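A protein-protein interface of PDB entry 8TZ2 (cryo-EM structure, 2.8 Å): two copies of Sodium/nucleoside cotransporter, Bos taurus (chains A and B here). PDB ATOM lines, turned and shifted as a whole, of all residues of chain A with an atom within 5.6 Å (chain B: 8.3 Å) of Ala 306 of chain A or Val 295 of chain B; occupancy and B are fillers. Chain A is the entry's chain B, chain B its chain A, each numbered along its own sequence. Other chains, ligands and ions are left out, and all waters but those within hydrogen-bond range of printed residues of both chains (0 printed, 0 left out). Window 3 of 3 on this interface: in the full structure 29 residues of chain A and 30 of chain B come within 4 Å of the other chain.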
ATOM      1  N   PHE A 296      -3.853 -21.941  24.988  1.00  0.00           N
ATOM      2  CA  PHE A 296      -4.980 -22.609  24.354  1.00  0.00           C
ATOM      3  C   PHE A 296      -5.493 -21.891  23.114  1.00  0.00           C
ATOM      4  O   PHE A 296      -6.487 -22.329  22.529  1.00  0.00           O
ATOM      5  CB  PHE A 296      -6.115 -22.776  25.364  1.00  0.00           C
ATOM      6  CG  PHE A 296      -5.713 -23.519  26.599  1.00  0.00           C
ATOM      7  CD1 PHE A 296      -5.288 -24.830  26.522  1.00  0.00           C
ATOM      8  CD2 PHE A 296      -5.756 -22.911  27.838  1.00  0.00           C
ATOM      9  CE1 PHE A 296      -4.917 -25.516  27.652  1.00  0.00           C
ATOM     10  CE2 PHE A 296      -5.387 -23.595  28.969  1.00  0.00           C
ATOM     11  CZ  PHE A 296      -4.969 -24.897  28.874  1.00  0.00           C
ATOM     12  N   HIS A 303     -14.141 -23.709  24.690  1.00  0.00           N
ATOM     13  CA  HIS A 303     -14.254 -24.569  25.865  1.00  0.00           C
ATOM     14  C   HIS A 303     -14.145 -23.633  27.060  1.00  0.00           C
ATOM     15  O   HIS A 303     -13.056 -23.397  27.587  1.00  0.00           O
ATOM     16  CB  HIS A 303     -13.184 -25.644  25.868  1.00  0.00           C
ATOM     17  CG  HIS A 303     -12.964 -26.278  24.531  1.00  0.00           C
ATOM     18  ND1 HIS A 303     -13.824 -27.215  24.000  1.00  0.00           N
ATOM     19  CD2 HIS A 303     -11.985 -26.105  23.616  1.00  0.00           C
ATOM     20  CE1 HIS A 303     -13.381 -27.592  22.814  1.00  0.00           C
ATOM     21  NE2 HIS A 303     -12.266 -26.933  22.557  1.00  0.00           N
ATOM     22  N   PHE A 304     -15.287 -23.095  27.482  1.00  0.00           N
ATOM     23  CA  PHE A 304     -15.272 -21.967  28.403  1.00  0.00           C
ATOM     24  C   PHE A 304     -14.700 -22.363  29.757  1.00  0.00           C
ATOM     25  O   PHE A 304     -13.725 -21.768  30.227  1.00  0.00           O
ATOM     26  CB  PHE A 304     -16.685 -21.405  28.551  1.00  0.00           C
ATOM     27  CG  PHE A 304     -16.807 -20.336  29.590  1.00  0.00           C
ATOM     28  CD1 PHE A 304     -16.390 -19.048  29.320  1.00  0.00           C
ATOM     29  CD2 PHE A 304     -17.345 -20.616  30.833  1.00  0.00           C
ATOM     30  CE1 PHE A 304     -16.499 -18.064  30.269  1.00  0.00           C
ATOM     31  CE2 PHE A 304     -17.456 -19.632  31.789  1.00  0.00           C
ATOM     32  CZ  PHE A 304     -17.034 -18.353  31.504  1.00  0.00           C
ATOM     33  N   PHE A 305     -15.263 -23.394  30.384  1.00  0.00           N
ATOM     34  CA  PHE A 305     -14.833 -23.725  31.734  1.00  0.00           C
ATOM     35  C   PHE A 305     -13.365 -24.134  31.760  1.00  0.00           C
ATOM     36  O   PHE A 305     -12.557 -23.510  32.457  1.00  0.00           O
ATOM     37  CB  PHE A 305     -15.716 -24.838  32.296  1.00  0.00           C
ATOM     38  CG  PHE A 305     -15.404 -25.206  33.712  1.00  0.00           C
ATOM     39  CD1 PHE A 305     -15.874 -24.442  34.760  1.00  0.00           C
ATOM     40  CD2 PHE A 305     -14.648 -26.326  33.995  1.00  0.00           C
ATOM     41  CE1 PHE A 305     -15.590 -24.783  36.058  1.00  0.00           C
ATOM     42  CE2 PHE A 305     -14.362 -26.670  35.290  1.00  0.00           C
ATOM     43  CZ  PHE A 305     -14.833 -25.899  36.325  1.00  0.00           C
ATOM     44  N   ALA A 306     -12.985 -25.104  30.929  1.00  0.00           N
ATOM     45  CA  ALA A 306     -11.668 -25.715  31.052  1.00  0.00           C
ATOM     46  C   ALA A 306     -10.558 -24.738  30.696  1.00  0.00           C
ATOM     47  O   ALA A 306      -9.511 -24.717  31.354  1.00  0.00           O
ATOM     48  CB  ALA A 306     -11.592 -26.957  30.169  1.00  0.00           C
ATOM     49  N   PHE A 307     -10.755 -23.932  29.656  1.00  0.00           N
ATOM     50  CA  PHE A 307      -9.703 -23.079  29.132  1.00  0.00           C
ATOM     51  C   PHE A 307      -9.862 -21.608  29.494  1.00  0.00           C
ATOM     52  O   PHE A 307      -9.054 -20.792  29.048  1.00  0.00           O
ATOM     53  CB  PHE A 307      -9.619 -23.221  27.610  1.00  0.00           C
ATOM     54  CG  PHE A 307      -9.152 -24.574  27.140  1.00  0.00           C
ATOM     55  CD1 PHE A 307      -8.753 -25.549  28.038  1.00  0.00           C
ATOM     56  CD2 PHE A 307      -9.102 -24.867  25.792  1.00  0.00           C
ATOM     57  CE1 PHE A 307      -8.324 -26.779  27.600  1.00  0.00           C
ATOM     58  CE2 PHE A 307      -8.671 -26.098  25.355  1.00  0.00           C
ATOM     59  CZ  PHE A 307      -8.282 -27.050  26.259  1.00  0.00           C
ATOM     60  N   LYS A 308     -10.872 -21.244  30.271  1.00  0.00           N
ATOM     61  CA  LYS A 308     -10.989 -19.866  30.732  1.00  0.00           C
ATOM     62  C   LYS A 308     -11.198 -19.748  32.235  1.00  0.00           C
ATOM     63  O   LYS A 308     -10.723 -18.782  32.832  1.00  0.00           O
ATOM     64  CB  LYS A 308     -12.127 -19.154  29.995  1.00  0.00           C
ATOM     65  CG  LYS A 308     -12.403 -17.764  30.505  1.00  0.00           C
ATOM     66  CD  LYS A 308     -12.969 -16.886  29.423  1.00  0.00           C
ATOM     67  CE  LYS A 308     -13.351 -15.531  29.969  1.00  0.00           C
ATOM     68  NZ  LYS A 308     -13.348 -14.493  28.907  1.00  0.00           N
ATOM     69  N   VAL A 309     -11.900 -20.691  32.856  1.00  0.00           N
ATOM     70  CA  VAL A 309     -12.236 -20.574  34.272  1.00  0.00           C
ATOM     71  C   VAL A 309     -11.131 -21.131  35.156  1.00  0.00           C
ATOM     72  O   VAL A 309     -10.733 -20.506  36.140  1.00  0.00           O
ATOM     73  CB  VAL A 309     -13.585 -21.272  34.540  1.00  0.00           C
ATOM     74  CG1 VAL A 309     -13.871 -21.343  36.021  1.00  0.00           C
ATOM     75  CG2 VAL A 309     -14.704 -20.543  33.827  1.00  0.00           C
ATOM     76  N   LEU A 310     -10.624 -22.317  34.831  1.00  0.00           N
ATOM     77  CA  LEU A 310      -9.539 -22.892  35.620  1.00  0.00           C
ATOM     78  C   LEU A 310      -8.280 -22.034  35.607  1.00  0.00           C
ATOM     79  O   LEU A 310      -7.624 -21.925  36.660  1.00  0.00           O
ATOM     80  CB  LEU A 310      -9.254 -24.310  35.119  1.00  0.00           C
ATOM     81  CG  LEU A 310     -10.424 -25.285  35.266  1.00  0.00           C
ATOM     82  CD1 LEU A 310     -10.084 -26.627  34.667  1.00  0.00           C
ATOM     83  CD2 LEU A 310     -10.816 -25.438  36.715  1.00  0.00           C
ATOM     84  N   PRO A 311      -7.880 -21.422  34.490  1.00  0.00           N
ATOM     85  CA  PRO A 311      -6.749 -20.487  34.541  1.00  0.00           C
ATOM     86  C   PRO A 311      -6.930 -19.378  35.561  1.00  0.00           C
ATOM     87  O   PRO A 311      -5.941 -18.899  36.128  1.00  0.00           O
ATOM     88  CB  PRO A 311      -6.694 -19.946  33.111  1.00  0.00           C
ATOM     89  CG  PRO A 311      -7.215 -21.047  32.285  1.00  0.00           C
ATOM     90  CD  PRO A 311      -8.261 -21.742  33.103  1.00  0.00           C
ATOM     91  N   ALA A 472     -12.078 -30.641  37.934  1.00  0.00           N
ATOM     92  CA  ALA A 472     -12.652 -31.071  36.666  1.00  0.00           C
ATOM     93  C   ALA A 472     -13.170 -32.501  36.743  1.00  0.00           C
ATOM     94  O   ALA A 472     -14.301 -32.787  36.322  1.00  0.00           O
ATOM     95  CB  ALA A 472     -11.606 -30.937  35.563  1.00  0.00           C
ATOM     96  N   LEU A 475     -16.302 -32.805  38.934  1.00  0.00           N
ATOM     97  CA  LEU A 475     -17.491 -32.305  38.258  1.00  0.00           C
ATOM     98  C   LEU A 475     -17.991 -33.296  37.217  1.00  0.00           C
ATOM     99  O   LEU A 475     -19.198 -33.561  37.136  1.00  0.00           O
ATOM    100  CB  LEU A 475     -17.192 -30.955  37.614  1.00  0.00           C
ATOM    101  CG  LEU A 475     -17.379 -29.737  38.510  1.00  0.00           C
ATOM    102  CD1 LEU A 475     -16.738 -28.513  37.899  1.00  0.00           C
ATOM    103  CD2 LEU A 475     -18.853 -29.510  38.713  1.00  0.00           C
ATOM    104  N   ILE A 476     -17.080 -33.873  36.431  1.00  0.00           N
ATOM    105  CA  ILE A 476     -17.502 -34.846  35.427  1.00  0.00           C
ATOM    106  C   ILE A 476     -18.253 -35.993  36.092  1.00  0.00           C
ATOM    107  O   ILE A 476     -19.376 -36.344  35.697  1.00  0.00           O
ATOM    108  CB  ILE A 476     -16.282 -35.365  34.641  1.00  0.00           C
ATOM    109  CG1 ILE A 476     -15.742 -34.309  33.682  1.00  0.00           C
ATOM    110  CG2 ILE A 476     -16.630 -36.625  33.896  1.00  0.00           C
ATOM    111  CD1 ILE A 476     -14.341 -34.589  33.227  1.00  0.00           C
ATOM    112  N   SER B 288     -21.842 -40.060  30.868  1.00  0.00           N
ATOM    113  CA  SER B 288     -20.660 -39.221  31.041  1.00  0.00           C
ATOM    114  C   SER B 288     -20.718 -37.959  30.192  1.00  0.00           C
ATOM    115  O   SER B 288     -20.014 -36.981  30.489  1.00  0.00           O
ATOM    116  CB  SER B 288     -19.414 -40.029  30.696  1.00  0.00           C
ATOM    117  OG  SER B 288     -19.476 -40.505  29.368  1.00  0.00           O
ATOM    118  N   ASP B 289     -21.543 -37.962  29.145  1.00  0.00           N
ATOM    119  CA  ASP B 289     -21.642 -36.803  28.271  1.00  0.00           C
ATOM    120  C   ASP B 289     -22.168 -35.589  29.016  1.00  0.00           C
ATOM    121  O   ASP B 289     -21.847 -34.458  28.650  1.00  0.00           O
ATOM    122  CB  ASP B 289     -22.540 -37.123  27.081  1.00  0.00           C
ATOM    123  CG  ASP B 289     -21.925 -38.140  26.143  1.00  0.00           C
ATOM    124  OD1 ASP B 289     -20.792 -38.592  26.411  1.00  0.00           O
ATOM    125  OD2 ASP B 289     -22.574 -38.489  25.137  1.00  0.00           O
ATOM    126  N   ALA B 290     -22.960 -35.799  30.065  1.00  0.00           N
ATOM    127  CA  ALA B 290     -23.481 -34.672  30.827  1.00  0.00           C
ATOM    128  C   ALA B 290     -22.358 -33.868  31.464  1.00  0.00           C
ATOM    129  O   ALA B 290     -22.364 -32.633  31.412  1.00  0.00           O
ATOM    130  CB  ALA B 290     -24.449 -35.172  31.892  1.00  0.00           C
ATOM    131  N   GLY B 291     -21.394 -34.546  32.084  1.00  0.00           N
ATOM    132  CA  GLY B 291     -20.255 -33.841  32.646  1.00  0.00           C
ATOM    133  C   GLY B 291     -19.297 -33.338  31.585  1.00  0.00           C
ATOM    134  O   GLY B 291     -18.743 -32.239  31.708  1.00  0.00           O
ATOM    135  N   ALA B 292     -19.073 -34.138  30.539  1.00  0.00           N
ATOM    136  CA  ALA B 292     -18.149 -33.711  29.494  1.00  0.00           C
ATOM    137  C   ALA B 292     -18.652 -32.456  28.791  1.00  0.00           C
ATOM    138  O   ALA B 292     -17.854 -31.597  28.402  1.00  0.00           O
ATOM    139  CB  ALA B 292     -17.920 -34.840  28.490  1.00  0.00           C
ATOM    140  N   SER B 293     -19.968 -32.329  28.622  1.00  0.00           N
ATOM    141  CA  SER B 293     -20.529 -31.169  27.945  1.00  0.00           C
ATOM    142  C   SER B 293     -20.375 -29.898  28.767  1.00  0.00           C
ATOM    143  O   SER B 293     -20.268 -28.807  28.198  1.00  0.00           O
ATOM    144  CB  SER B 293     -22.001 -31.419  27.627  1.00  0.00           C
ATOM    145  OG  SER B 293     -22.556 -30.347  26.889  1.00  0.00           O
ATOM    146  N   PHE B 294     -20.377 -30.007  30.095  1.00  0.00           N
ATOM    147  CA  PHE B 294     -20.165 -28.823  30.916  1.00  0.00           C
ATOM    148  C   PHE B 294     -18.689 -28.474  31.014  1.00  0.00           C
ATOM    149  O   PHE B 294     -18.300 -27.329  30.767  1.00  0.00           O
ATOM    150  CB  PHE B 294     -20.740 -29.021  32.316  1.00  0.00           C
ATOM    151  CG  PHE B 294     -20.385 -27.912  33.260  1.00  0.00           C
ATOM    152  CD1 PHE B 294     -20.938 -26.656  33.102  1.00  0.00           C
ATOM    153  CD2 PHE B 294     -19.483 -28.116  34.287  1.00  0.00           C
ATOM    154  CE1 PHE B 294     -20.606 -25.631  33.954  1.00  0.00           C
ATOM    155  CE2 PHE B 294     -19.152 -27.092  35.142  1.00  0.00           C
ATOM    156  CZ  PHE B 294     -19.713 -25.849  34.975  1.00  0.00           C
ATOM    157  N   VAL B 295     -17.848 -29.444  31.379  1.00  0.00           N
ATOM    158  CA  VAL B 295     -16.435 -29.139  31.576  1.00  0.00           C
ATOM    159  C   VAL B 295     -15.807 -28.652  30.277  1.00  0.00           C
ATOM    160  O   VAL B 295     -15.020 -27.699  30.272  1.00  0.00           O
ATOM    161  CB  VAL B 295     -15.694 -30.362  32.149  1.00  0.00           C
ATOM    162  CG1 VAL B 295     -14.207 -30.095  32.241  1.00  0.00           C
ATOM    163  CG2 VAL B 295     -16.230 -30.718  33.514  1.00  0.00           C
ATOM    164  N   PHE B 296     -16.150 -29.286  29.158  1.00  0.00           N
ATOM    165  CA  PHE B 296     -15.521 -29.007  27.875  1.00  0.00           C
ATOM    166  C   PHE B 296     -16.462 -28.365  26.865  1.00  0.00           C
ATOM    167  O   PHE B 296     -16.058 -28.141  25.721  1.00  0.00           O
ATOM    168  CB  PHE B 296     -14.939 -30.296  27.296  1.00  0.00           C
ATOM    169  CG  PHE B 296     -13.962 -30.974  28.204  1.00  0.00           C
ATOM    170  CD1 PHE B 296     -12.789 -30.342  28.568  1.00  0.00           C
ATOM    171  CD2 PHE B 296     -14.212 -32.238  28.697  1.00  0.00           C
ATOM    172  CE1 PHE B 296     -11.890 -30.959  29.402  1.00  0.00           C
ATOM    173  CE2 PHE B 296     -13.313 -32.857  29.530  1.00  0.00           C
ATOM    174  CZ  PHE B 296     -12.154 -32.216  29.882  1.00  0.00           C
ATOM    175  N   GLY B 297     -17.698 -28.076  27.249  1.00  0.00           N
ATOM    176  CA  GLY B 297     -18.608 -27.337  26.403  1.00  0.00           C
ATOM    177  C   GLY B 297     -19.340 -28.206  25.403  1.00  0.00           C
ATOM    178  O   GLY B 297     -19.121 -29.409  25.278  1.00  0.00           O
ATOM    179  N   GLU B 298     -20.245 -27.557  24.667  1.00  0.00           N
ATOM    180  CA  GLU B 298     -20.999 -28.229  23.619  1.00  0.00           C
ATOM    181  C   GLU B 298     -20.133 -28.610  22.428  1.00  0.00           C
ATOM    182  O   GLU B 298     -20.586 -29.382  21.577  1.00  0.00           O
ATOM    183  CB  GLU B 298     -22.148 -27.340  23.152  1.00  0.00           C
ATOM    184  CG  GLU B 298     -23.202 -27.089  24.217  1.00  0.00           C
ATOM    185  CD  GLU B 298     -24.331 -26.205  23.724  1.00  0.00           C
ATOM    186  OE1 GLU B 298     -24.259 -25.736  22.569  1.00  0.00           O
ATOM    187  OE2 GLU B 298     -25.291 -25.981  24.491  1.00  0.00           O
ATOM    188  N   TYR B 300     -17.343 -30.260  22.821  1.00  0.00           N
ATOM    189  CA  TYR B 300     -16.482 -31.333  23.295  1.00  0.00           C
ATOM    190  C   TYR B 300     -16.333 -32.440  22.263  1.00  0.00           C
ATOM    191  O   TYR B 300     -15.396 -33.240  22.358  1.00  0.00           O
ATOM    192  CB  TYR B 300     -17.026 -31.893  24.612  1.00  0.00           C
ATOM    193  CG  TYR B 300     -18.289 -32.711  24.489  1.00  0.00           C
ATOM    194  CD1 TYR B 300     -19.494 -32.120  24.150  1.00  0.00           C
ATOM    195  CD2 TYR B 300     -18.280 -34.071  24.740  1.00  0.00           C
ATOM    196  CE1 TYR B 300     -20.644 -32.863  24.045  1.00  0.00           C
ATOM    197  CE2 TYR B 300     -19.425 -34.821  24.637  1.00  0.00           C
ATOM    198  CZ  TYR B 300     -20.606 -34.212  24.290  1.00  0.00           C
ATOM    199  OH  TYR B 300     -21.755 -34.958  24.188  1.00  0.00           O
ATOM    200  N   PHE B 307     -12.063 -35.564  25.002  1.00  0.00           N
ATOM    201  CA  PHE B 307     -13.162 -34.932  25.711  1.00  0.00           C
ATOM    202  C   PHE B 307     -14.448 -35.746  25.708  1.00  0.00           C
ATOM    203  O   PHE B 307     -15.458 -35.270  26.231  1.00  0.00           O
ATOM    204  CB  PHE B 307     -13.437 -33.545  25.124  1.00  0.00           C
ATOM    205  CG  PHE B 307     -12.333 -32.546  25.357  1.00  0.00           C
ATOM    206  CD1 PHE B 307     -11.222 -32.865  26.119  1.00  0.00           C
ATOM    207  CD2 PHE B 307     -12.415 -31.277  24.818  1.00  0.00           C
ATOM    208  CE1 PHE B 307     -10.222 -31.946  26.328  1.00  0.00           C
ATOM    209  CE2 PHE B 307     -11.414 -30.358  25.030  1.00  0.00           C
ATOM    210  CZ  PHE B 307     -10.321 -30.694  25.785  1.00  0.00           C
ATOM    211  N   PRO B 311     -13.592 -39.285  29.665  1.00  0.00           N
ATOM    212  CA  PRO B 311     -14.630 -39.140  30.695  1.00  0.00           C
ATOM    213  C   PRO B 311     -15.397 -40.423  30.962  1.00  0.00           C
ATOM    214  O   PRO B 311     -15.843 -40.645  32.094  1.00  0.00           O
ATOM    215  CB  PRO B 311     -15.529 -38.046  30.115  1.00  0.00           C
ATOM    216  CG  PRO B 311     -14.622 -37.223  29.299  1.00  0.00           C
ATOM    217  CD  PRO B 311     -13.599 -38.154  28.722  1.00  0.00           C
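The backbone carbonyl oxygen (O) of Val 295 of chain B sits at hydrogen-bond distance from the backbone NH (N) of Ala 306 of chain A (3.4 Å).
O of Phe 296 of chain B lies within hydrogen-bond range of ND1 of His 303 of chain A (3.0 Å).
The backbone carbonyl oxygen (O) of Phe 305 of chain A sits at hydrogen-bond distance from the backbone NH (N) of Leu 310 of chain A, 3.3 Å away.
Among the printed residues, pairs that only touch across the chains: Phe 305 of chain A with Phe 294 of chain B (3.9 Å), Phe 305 of chain A with Val 295 of chain B (3.6 Å), Ala 306 of chain A with Phe 296 of chain B (3.9 Å), Ala 472 of chain A with Val 295 of chain B (3.99 Å), Leu 475 of chain A with Phe 294 of chain B (3.9 Å) and Ile 476 of chain A with Val 295 of chain B (3.6 Å).
Of chain B, only Val 295 (3.4 Å) and Phe 296 (3.9 Å) come within 4 Å of Ala 306 of chain A.
Printed residues of chain A within 4 Å of Val 295 of chain B: Phe 305, Ala 306, Ala 472 and Ile 476.
Printed residues of chain B within 4 Å of His 303 of chain A: Phe 296.
Printed residues of chain B within 4 Å of Phe 305 of chain A: Phe 294 and Val 295.
Of the printed residues of chain A, Phe 296 of chain B touches His 303 (3.0 Å) and Ala 306 (3.9 Å).
The nearest residue of chain B that does not touch Ala 306 of chain A is Phe 294 of chain B (5.8 Å).
The nearest printed residue of chain A that does not touch Val 295 of chain B is Leu 475 of chain A (4.2 Å).
The nearest printed residue of chain B that does not touch His 303 of chain A is Phe 307 of chain B (4.1 Å).
Hydrophobic or aromatic side chains of chain A within 4 Å of the printed part of chain B: His 303, Phe 305, Ala 306, Leu 475 and Ile 476.
Of the 14 printed residues of chain B, 3 touch a printed residue of chain A.
Hydrophobic or aromatic side chains of chain B within 4 Å of the printed part of chain A: Phe 294, Val 295 and Phe 296.
Among the printed residues, no Asp or Glu carboxylate lies within 4 Å of a Lys or Arg side-chain nitrogen of the other chain.
3 positions are printed for both chains.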
